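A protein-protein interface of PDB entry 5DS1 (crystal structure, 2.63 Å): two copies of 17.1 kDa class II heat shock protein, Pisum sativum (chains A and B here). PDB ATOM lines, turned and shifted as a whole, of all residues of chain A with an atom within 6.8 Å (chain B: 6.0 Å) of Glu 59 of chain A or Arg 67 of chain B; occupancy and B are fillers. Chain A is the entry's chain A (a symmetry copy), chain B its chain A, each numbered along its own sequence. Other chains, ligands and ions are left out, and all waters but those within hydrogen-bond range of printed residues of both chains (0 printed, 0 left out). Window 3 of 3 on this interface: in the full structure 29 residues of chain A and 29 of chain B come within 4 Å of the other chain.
Of chain B, only Ala 5, Asp 6 and Arg 67 come within 4 Å of Glu 59 of chain A. Of chain A, only Glu 59 (3.0 Å) comes within 4 Å of Arg 67 of chain B. Printed residues of chain A within 4 Å of Ala 5 of chain B: Glu 59 and Arg 60. Printed residues of chain B within 4 Å of Met 58 of chain A: Asp 6 (3.3 Å). Of the printed residues of chain B, Lys 57 of chain A touches Asp 6 (3.2 Å). Of the printed residues of chain B, Arg 60 of chain A touches Pro 4 (3.96 Å), Ala 5 (3.98 Å) and Asp 6 (2.9 Å). Met 66 of chain B touches none of the printed residues of chain A. The nearest residue of chain A that does not touch Arg 67 of chain B is Lys 57 of chain A (4.5 Å).
Among the printed residues, Asp or Glu carboxylates within 4 Å of a Lys or Arg side-chain nitrogen of the other chain: Glu 59 of chain A with Arg 67 of chain B (3.0 Å) and Arg 60 of chain A with Asp 6 of chain B (3.1 Å).
N of Glu 59 of chain A is in hydrogen-bond range of O of Ala 5 of chain B, 3.2 Å away. The guanidinium group (NH1) of Arg 67 of chain B lies within salt-bridge range of the side-chain carboxylate (OE2) of Glu 59 of chain A, 3.0 Å away. The guanidinium group (NE) of Arg 60 of chain A is in salt-bridge range of the side-chain carboxylate (OD2) of Asp 6 of chain B. OD1 of Asp 6 of chain B lies within hydrogen-bond range of N of Glu 59 of chain A.
Lys 57 of chain A touches Asp 6 of chain B (O to CA, 3.2 Å). CA of Met 58 of chain A touches OD1 of Asp 6 of chain B (3.3 Å). Pro 4 of chain B touches Arg 60 of chain A (CB to CG, 3.96 Å). Ala 5 of chain B touches Arg 60 of chain A.
The backbone carbonyl oxygen of Arg 67 of chain B sits at hydrogen-bond distance from the backbone NH of Ile 40 of chain B (2.9 Å). The side-chain carboxylate (OE1) of Glu 59 of chain A is in salt-bridge range of the side-chain amino group (NZ) of Lys 57 of chain A (2.9 Å). NH1 of Arg 67 of chain B lies within hydrogen-bond range of O of Thr 3 of chain B.
No position is printed for both chains.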
ATOM      1  N   ARG A  44      -3.495   0.633 -11.829  1.00  0.00           N
ATOM      2  CA  ARG A  44      -3.813   0.654 -10.405  1.00  0.00           C
ATOM      3  C   ARG A  44      -5.310   0.458 -10.213  1.00  0.00           C
ATOM      4  O   ARG A  44      -6.129   1.073 -10.914  1.00  0.00           O
ATOM      5  CB  ARG A  44      -3.378   1.967  -9.744  1.00  0.00           C
ATOM      6  CG  ARG A  44      -2.270   2.720 -10.449  1.00  0.00           C
ATOM      7  CD  ARG A  44      -2.234   4.155  -9.985  1.00  0.00           C
ATOM      8  NE  ARG A  44      -1.685   4.245  -8.639  1.00  0.00           N
ATOM      9  CZ  ARG A  44      -1.980   5.200  -7.763  1.00  0.00           C
ATOM     10  NH1 ARG A  44      -2.842   6.157  -8.073  1.00  0.00           N
ATOM     11  NH2 ARG A  44      -1.416   5.188  -6.566  1.00  0.00           N
ATOM     12  N   LYS A  57     -11.319  10.541   2.303  1.00  0.00           N
ATOM     13  CA  LYS A  57     -10.587  11.319   1.329  1.00  0.00           C
ATOM     14  C   LYS A  57     -10.053  10.362   0.287  1.00  0.00           C
ATOM     15  O   LYS A  57      -9.587   9.257   0.609  1.00  0.00           O
ATOM     16  CB  LYS A  57      -9.454  12.136   1.966  1.00  0.00           C
ATOM     17  CG  LYS A  57      -9.933  13.507   2.451  1.00  0.00           C
ATOM     18  CD  LYS A  57      -8.813  14.344   3.073  1.00  0.00           C
ATOM     19  CE  LYS A  57      -9.011  15.822   2.750  1.00  0.00           C
ATOM     20  NZ  LYS A  57      -8.025  16.330   1.738  1.00  0.00           N
ATOM     21  N   MET A  58     -10.166  10.789  -0.969  1.00  0.00           N
ATOM     22  CA  MET A  58      -9.755   9.973  -2.101  1.00  0.00           C
ATOM     23  C   MET A  58      -9.072  10.915  -3.076  1.00  0.00           C
ATOM     24  O   MET A  58      -9.739  11.630  -3.827  1.00  0.00           O
ATOM     25  CB  MET A  58     -10.943   9.271  -2.735  1.00  0.00           C
ATOM     26  CG  MET A  58     -10.677   7.841  -3.092  1.00  0.00           C
ATOM     27  SD  MET A  58     -12.144   7.216  -3.899  1.00  0.00           S
ATOM     28  CE  MET A  58     -12.003   8.082  -5.453  1.00  0.00           C
ATOM     29  N   GLU A  59      -7.747  10.916  -3.060  1.00  0.00           N
ATOM     30  CA  GLU A  59      -6.988  11.693  -4.021  1.00  0.00           C
ATOM     31  C   GLU A  59      -6.090  10.859  -4.934  1.00  0.00           C
ATOM     32  O   GLU A  59      -5.533  11.414  -5.881  1.00  0.00           O
ATOM     33  CB  GLU A  59      -6.164  12.764  -3.288  1.00  0.00           C
ATOM     34  CG  GLU A  59      -6.922  13.296  -2.086  1.00  0.00           C
ATOM     35  CD  GLU A  59      -6.144  14.310  -1.275  1.00  0.00           C
ATOM     36  OE1 GLU A  59      -6.773  15.027  -0.470  1.00  0.00           O
ATOM     37  OE2 GLU A  59      -4.921  14.394  -1.473  1.00  0.00           O
ATOM     38  N   ARG A  60      -5.932   9.558  -4.699  1.00  0.00           N
ATOM     39  CA  ARG A  60      -5.144   8.721  -5.601  1.00  0.00           C
ATOM     40  C   ARG A  60      -6.016   8.290  -6.774  1.00  0.00           C
ATOM     41  O   ARG A  60      -6.955   7.507  -6.599  1.00  0.00           O
ATOM     42  CB  ARG A  60      -4.577   7.485  -4.904  1.00  0.00           C
ATOM     43  CG  ARG A  60      -3.983   7.678  -3.484  1.00  0.00           C
ATOM     44  CD  ARG A  60      -3.125   6.421  -3.138  1.00  0.00           C
ATOM     45  NE  ARG A  60      -3.949   5.262  -3.383  1.00  0.00           N
ATOM     46  CZ  ARG A  60      -3.507   4.086  -3.808  1.00  0.00           C
ATOM     47  NH1 ARG A  60      -2.213   3.885  -4.065  1.00  0.00           N
ATOM     48  NH2 ARG A  60      -4.375   3.090  -3.997  1.00  0.00           N
ATOM     49  N   ARG A  61      -5.711   8.801  -7.963  1.00  0.00           N
ATOM     50  CA  ARG A  61      -6.395   8.355  -9.165  1.00  0.00           C
ATOM     51  C   ARG A  61      -5.890   6.977  -9.566  1.00  0.00           C
ATOM     52  O   ARG A  61      -4.724   6.636  -9.365  1.00  0.00           O
ATOM     53  CB  ARG A  61      -6.203   9.344 -10.323  1.00  0.00           C
ATOM     54  CG  ARG A  61      -7.401  10.284 -10.555  1.00  0.00           C
ATOM     55  CD  ARG A  61      -7.124  11.244 -11.700  1.00  0.00           C
ATOM     56  NE  ARG A  61      -6.153  10.663 -12.622  1.00  0.00           N
ATOM     57  CZ  ARG A  61      -6.461   9.863 -13.637  1.00  0.00           C
ATOM     58  NH1 ARG A  61      -5.499   9.378 -14.412  1.00  0.00           N
ATOM     59  NH2 ARG A  61      -7.727   9.552 -13.884  1.00  0.00           N
ATOM     60  N   SER B   2       4.646  17.045  -1.023  1.00  0.00           N
ATOM     61  CA  SER B   2       3.301  16.458  -0.999  1.00  0.00           C
ATOM     62  C   SER B   2       3.137  15.244  -1.914  1.00  0.00           C
ATOM     63  O   SER B   2       3.916  15.057  -2.848  1.00  0.00           O
ATOM     64  CB  SER B   2       2.264  17.491  -1.398  1.00  0.00           C
ATOM     65  OG  SER B   2       1.015  16.845  -1.543  1.00  0.00           O
ATOM     66  N   THR B   3       2.092  14.446  -1.671  1.00  0.00           N
ATOM     67  CA  THR B   3       1.903  13.205  -2.415  1.00  0.00           C
ATOM     68  C   THR B   3       0.484  12.679  -2.222  1.00  0.00           C
ATOM     69  O   THR B   3      -0.138  12.949  -1.185  1.00  0.00           O
ATOM     70  CB  THR B   3       2.950  12.178  -1.966  1.00  0.00           C
ATOM     71  OG1 THR B   3       2.793  10.932  -2.675  1.00  0.00           O
ATOM     72  CG2 THR B   3       2.858  11.948  -0.454  1.00  0.00           C
ATOM     73  N   PRO B   4      -0.068  11.942  -3.197  1.00  0.00           N
ATOM     74  CA  PRO B   4      -1.474  11.528  -3.126  1.00  0.00           C
ATOM     75  C   PRO B   4      -1.779  10.646  -1.920  1.00  0.00           C
ATOM     76  O   PRO B   4      -1.012   9.741  -1.589  1.00  0.00           O
ATOM     77  CB  PRO B   4      -1.667  10.748  -4.431  1.00  0.00           C
ATOM     78  CG  PRO B   4      -0.664  11.304  -5.328  1.00  0.00           C
ATOM     79  CD  PRO B   4       0.513  11.585  -4.505  1.00  0.00           C
ATOM     80  N   ALA B   5      -2.952  10.874  -1.312  1.00  0.00           N
ATOM     81  CA  ALA B   5      -3.422  10.105  -0.159  1.00  0.00           C
ATOM     82  C   ALA B   5      -4.912   9.787  -0.236  1.00  0.00           C
ATOM     83  O   ALA B   5      -5.730  10.638  -0.605  1.00  0.00           O
ATOM     84  CB  ALA B   5      -3.164  10.852   1.148  1.00  0.00           C
ATOM     85  N   ASP B   6      -5.260   8.560   0.133  1.00  0.00           N
ATOM     86  CA  ASP B   6      -6.636   8.160   0.369  1.00  0.00           C
ATOM     87  C   ASP B   6      -6.810   7.917   1.863  1.00  0.00           C
ATOM     88  O   ASP B   6      -5.859   7.547   2.551  1.00  0.00           O
ATOM     89  CB  ASP B   6      -7.002   6.882  -0.396  1.00  0.00           C
ATOM     90  CG  ASP B   6      -6.948   7.038  -1.911  1.00  0.00           C
ATOM     91  OD1 ASP B   6      -7.011   8.174  -2.442  1.00  0.00           O
ATOM     92  OD2 ASP B   6      -6.854   5.982  -2.566  1.00  0.00           O
ATOM     93  N   VAL B  18      -0.875   6.197   1.124  1.00  0.00           N
ATOM     94  CA  VAL B  18      -0.049   7.246   0.548  1.00  0.00           C
ATOM     95  C   VAL B  18       0.791   6.645  -0.583  1.00  0.00           C
ATOM     96  O   VAL B  18       1.345   5.557  -0.429  1.00  0.00           O
ATOM     97  CB  VAL B  18       0.838   7.888   1.627  1.00  0.00           C
ATOM     98  CG1 VAL B  18       1.511   9.126   1.091  1.00  0.00           C
ATOM     99  CG2 VAL B  18      -0.004   8.200   2.885  1.00  0.00           C
ATOM    100  N   LEU B  38      -1.072  12.677  12.796  1.00  0.00           N
ATOM    101  CA  LEU B  38      -0.305  11.589  12.215  1.00  0.00           C
ATOM    102  C   LEU B  38       0.539  12.164  11.076  1.00  0.00           C
ATOM    103  O   LEU B  38       0.021  12.851  10.193  1.00  0.00           O
ATOM    104  CB  LEU B  38      -1.231  10.474  11.731  1.00  0.00           C
ATOM    105  CG  LEU B  38      -0.597   9.402  10.850  1.00  0.00           C
ATOM    106  CD1 LEU B  38       0.313   8.483  11.643  1.00  0.00           C
ATOM    107  CD2 LEU B  38      -1.657   8.605  10.144  1.00  0.00           C
ATOM    108  N   LEU B  39       1.837  11.902  11.109  1.00  0.00           N
ATOM    109  CA  LEU B  39       2.788  12.545  10.218  1.00  0.00           C
ATOM    110  C   LEU B  39       3.476  11.466   9.399  1.00  0.00           C
ATOM    111  O   LEU B  39       4.219  10.636   9.947  1.00  0.00           O
ATOM    112  CB  LEU B  39       3.792  13.365  11.017  1.00  0.00           C
ATOM    113  CG  LEU B  39       4.890  14.132  10.313  1.00  0.00           C
ATOM    114  CD1 LEU B  39       5.240  15.335  11.149  1.00  0.00           C
ATOM    115  CD2 LEU B  39       6.120  13.291  10.118  1.00  0.00           C
ATOM    116  N   ILE B  40       3.239  11.476   8.090  1.00  0.00           N
ATOM    117  CA  ILE B  40       3.745  10.439   7.196  1.00  0.00           C
ATOM    118  C   ILE B  40       4.761  11.074   6.250  1.00  0.00           C
ATOM    119  O   ILE B  40       4.530  12.166   5.717  1.00  0.00           O
ATOM    120  CB  ILE B  40       2.590   9.720   6.468  1.00  0.00           C
ATOM    121  CG1 ILE B  40       1.779   8.963   7.533  1.00  0.00           C
ATOM    122  CG2 ILE B  40       3.116   8.718   5.514  1.00  0.00           C
ATOM    123  CD1 ILE B  40       0.699   8.035   7.061  1.00  0.00           C
ATOM    124  N   SER B  41       5.912  10.421   6.094  1.00  0.00           N
ATOM    125  CA  SER B  41       7.060  11.051   5.455  1.00  0.00           C
ATOM    126  C   SER B  41       7.933   9.995   4.778  1.00  0.00           C
ATOM    127  O   SER B  41       8.124   8.906   5.326  1.00  0.00           O
ATOM    128  CB  SER B  41       7.849  11.855   6.500  1.00  0.00           C
ATOM    129  OG  SER B  41       9.234  11.821   6.257  1.00  0.00           O
ATOM    130  N   LEU B  65       8.574  13.265   0.231  1.00  0.00           N
ATOM    131  CA  LEU B  65       7.119  13.302   0.230  1.00  0.00           C
ATOM    132  C   LEU B  65       6.654  13.362   1.683  1.00  0.00           C
ATOM    133  O   LEU B  65       7.206  12.666   2.539  1.00  0.00           O
ATOM    134  CB  LEU B  65       6.576  12.054  -0.464  1.00  0.00           C
ATOM    135  CG  LEU B  65       7.287  11.664  -1.764  1.00  0.00           C
ATOM    136  CD1 LEU B  65       6.694  10.426  -2.355  1.00  0.00           C
ATOM    137  CD2 LEU B  65       7.226  12.766  -2.788  1.00  0.00           C
ATOM    138  N   MET B  66       5.661  14.194   1.972  1.00  0.00           N
ATOM    139  CA  MET B  66       5.192  14.335   3.347  1.00  0.00           C
ATOM    140  C   MET B  66       3.737  14.774   3.362  1.00  0.00           C
ATOM    141  O   MET B  66       3.331  15.636   2.576  1.00  0.00           O
ATOM    142  CB  MET B  66       6.054  15.335   4.124  1.00  0.00           C
ATOM    143  CG  MET B  66       5.457  15.809   5.426  1.00  0.00           C
ATOM    144  SD  MET B  66       6.320  17.283   5.995  1.00  0.00           S
ATOM    145  CE  MET B  66       7.986  16.649   6.182  1.00  0.00           C
ATOM    146  N   ARG B  67       2.952  14.163   4.251  1.00  0.00           N
ATOM    147  CA  ARG B  67       1.576  14.572   4.500  1.00  0.00           C
ATOM    148  C   ARG B  67       1.275  14.441   5.982  1.00  0.00           C
ATOM    149  O   ARG B  67       1.703  13.484   6.630  1.00  0.00           O
ATOM    150  CB  ARG B  67       0.572  13.739   3.693  1.00  0.00           C
ATOM    151  CG  ARG B  67       0.694  13.915   2.177  1.00  0.00           C
ATOM    152  CD  ARG B  67      -0.171  15.053   1.646  1.00  0.00           C
ATOM    153  NE  ARG B  67      -1.487  15.109   2.276  1.00  0.00           N
ATOM    154  CZ  ARG B  67      -2.621  14.870   1.632  1.00  0.00           C
ATOM    155  NH1 ARG B  67      -2.571  14.545   0.348  1.00  0.00           N
ATOM    156  NH2 ARG B  67      -3.797  14.955   2.257  1.00  0.00           N
ATOM    157  N   LYS B  68       0.556  15.416   6.511  1.00  0.00           N
ATOM    158  CA  LYS B  68       0.077  15.391   7.879  1.00  0.00           C
ATOM    159  C   LYS B  68      -1.413  15.099   7.882  1.00  0.00           C
ATOM    160  O   LYS B  68      -2.139  15.493   6.966  1.00  0.00           O
ATOM    161  CB  LYS B  68       0.350  16.722   8.577  1.00  0.00           C
ATOM    162  CG  LYS B  68       1.842  17.048   8.685  1.00  0.00           C
ATOM    163  CD  LYS B  68       2.076  18.446   9.271  1.00  0.00           C
ATOM    164  CE  LYS B  68       3.510  18.935   9.028  1.00  0.00           C
ATOM    165  NZ  LYS B  68       3.707  20.308   9.574  1.00  0.00           N
ATOM    166  N   PHE B  69      -1.857  14.381   8.908  1.00  0.00           N
ATOM    167  CA  PHE B  69      -3.267  14.064   9.089  1.00  0.00           C
ATOM    168  C   PHE B  69      -3.636  14.245  10.548  1.00  0.00           C
ATOM    169  O   PHE B  69      -3.025  13.627  11.431  1.00  0.00           O
ATOM    170  CB  PHE B  69      -3.596  12.634   8.662  1.00  0.00           C
ATOM    171  CG  PHE B  69      -3.306  12.363   7.253  1.00  0.00           C
ATOM    172  CD1 PHE B  69      -4.228  12.721   6.274  1.00  0.00           C
ATOM    173  CD2 PHE B  69      -2.134  11.744   6.886  1.00  0.00           C
ATOM    174  CE1 PHE B  69      -3.975  12.462   4.931  1.00  0.00           C
ATOM    175  CE2 PHE B  69      -1.864  11.475   5.566  1.00  0.00           C
ATOM    176  CZ  PHE B  69      -2.786  11.827   4.583  1.00  0.00           C
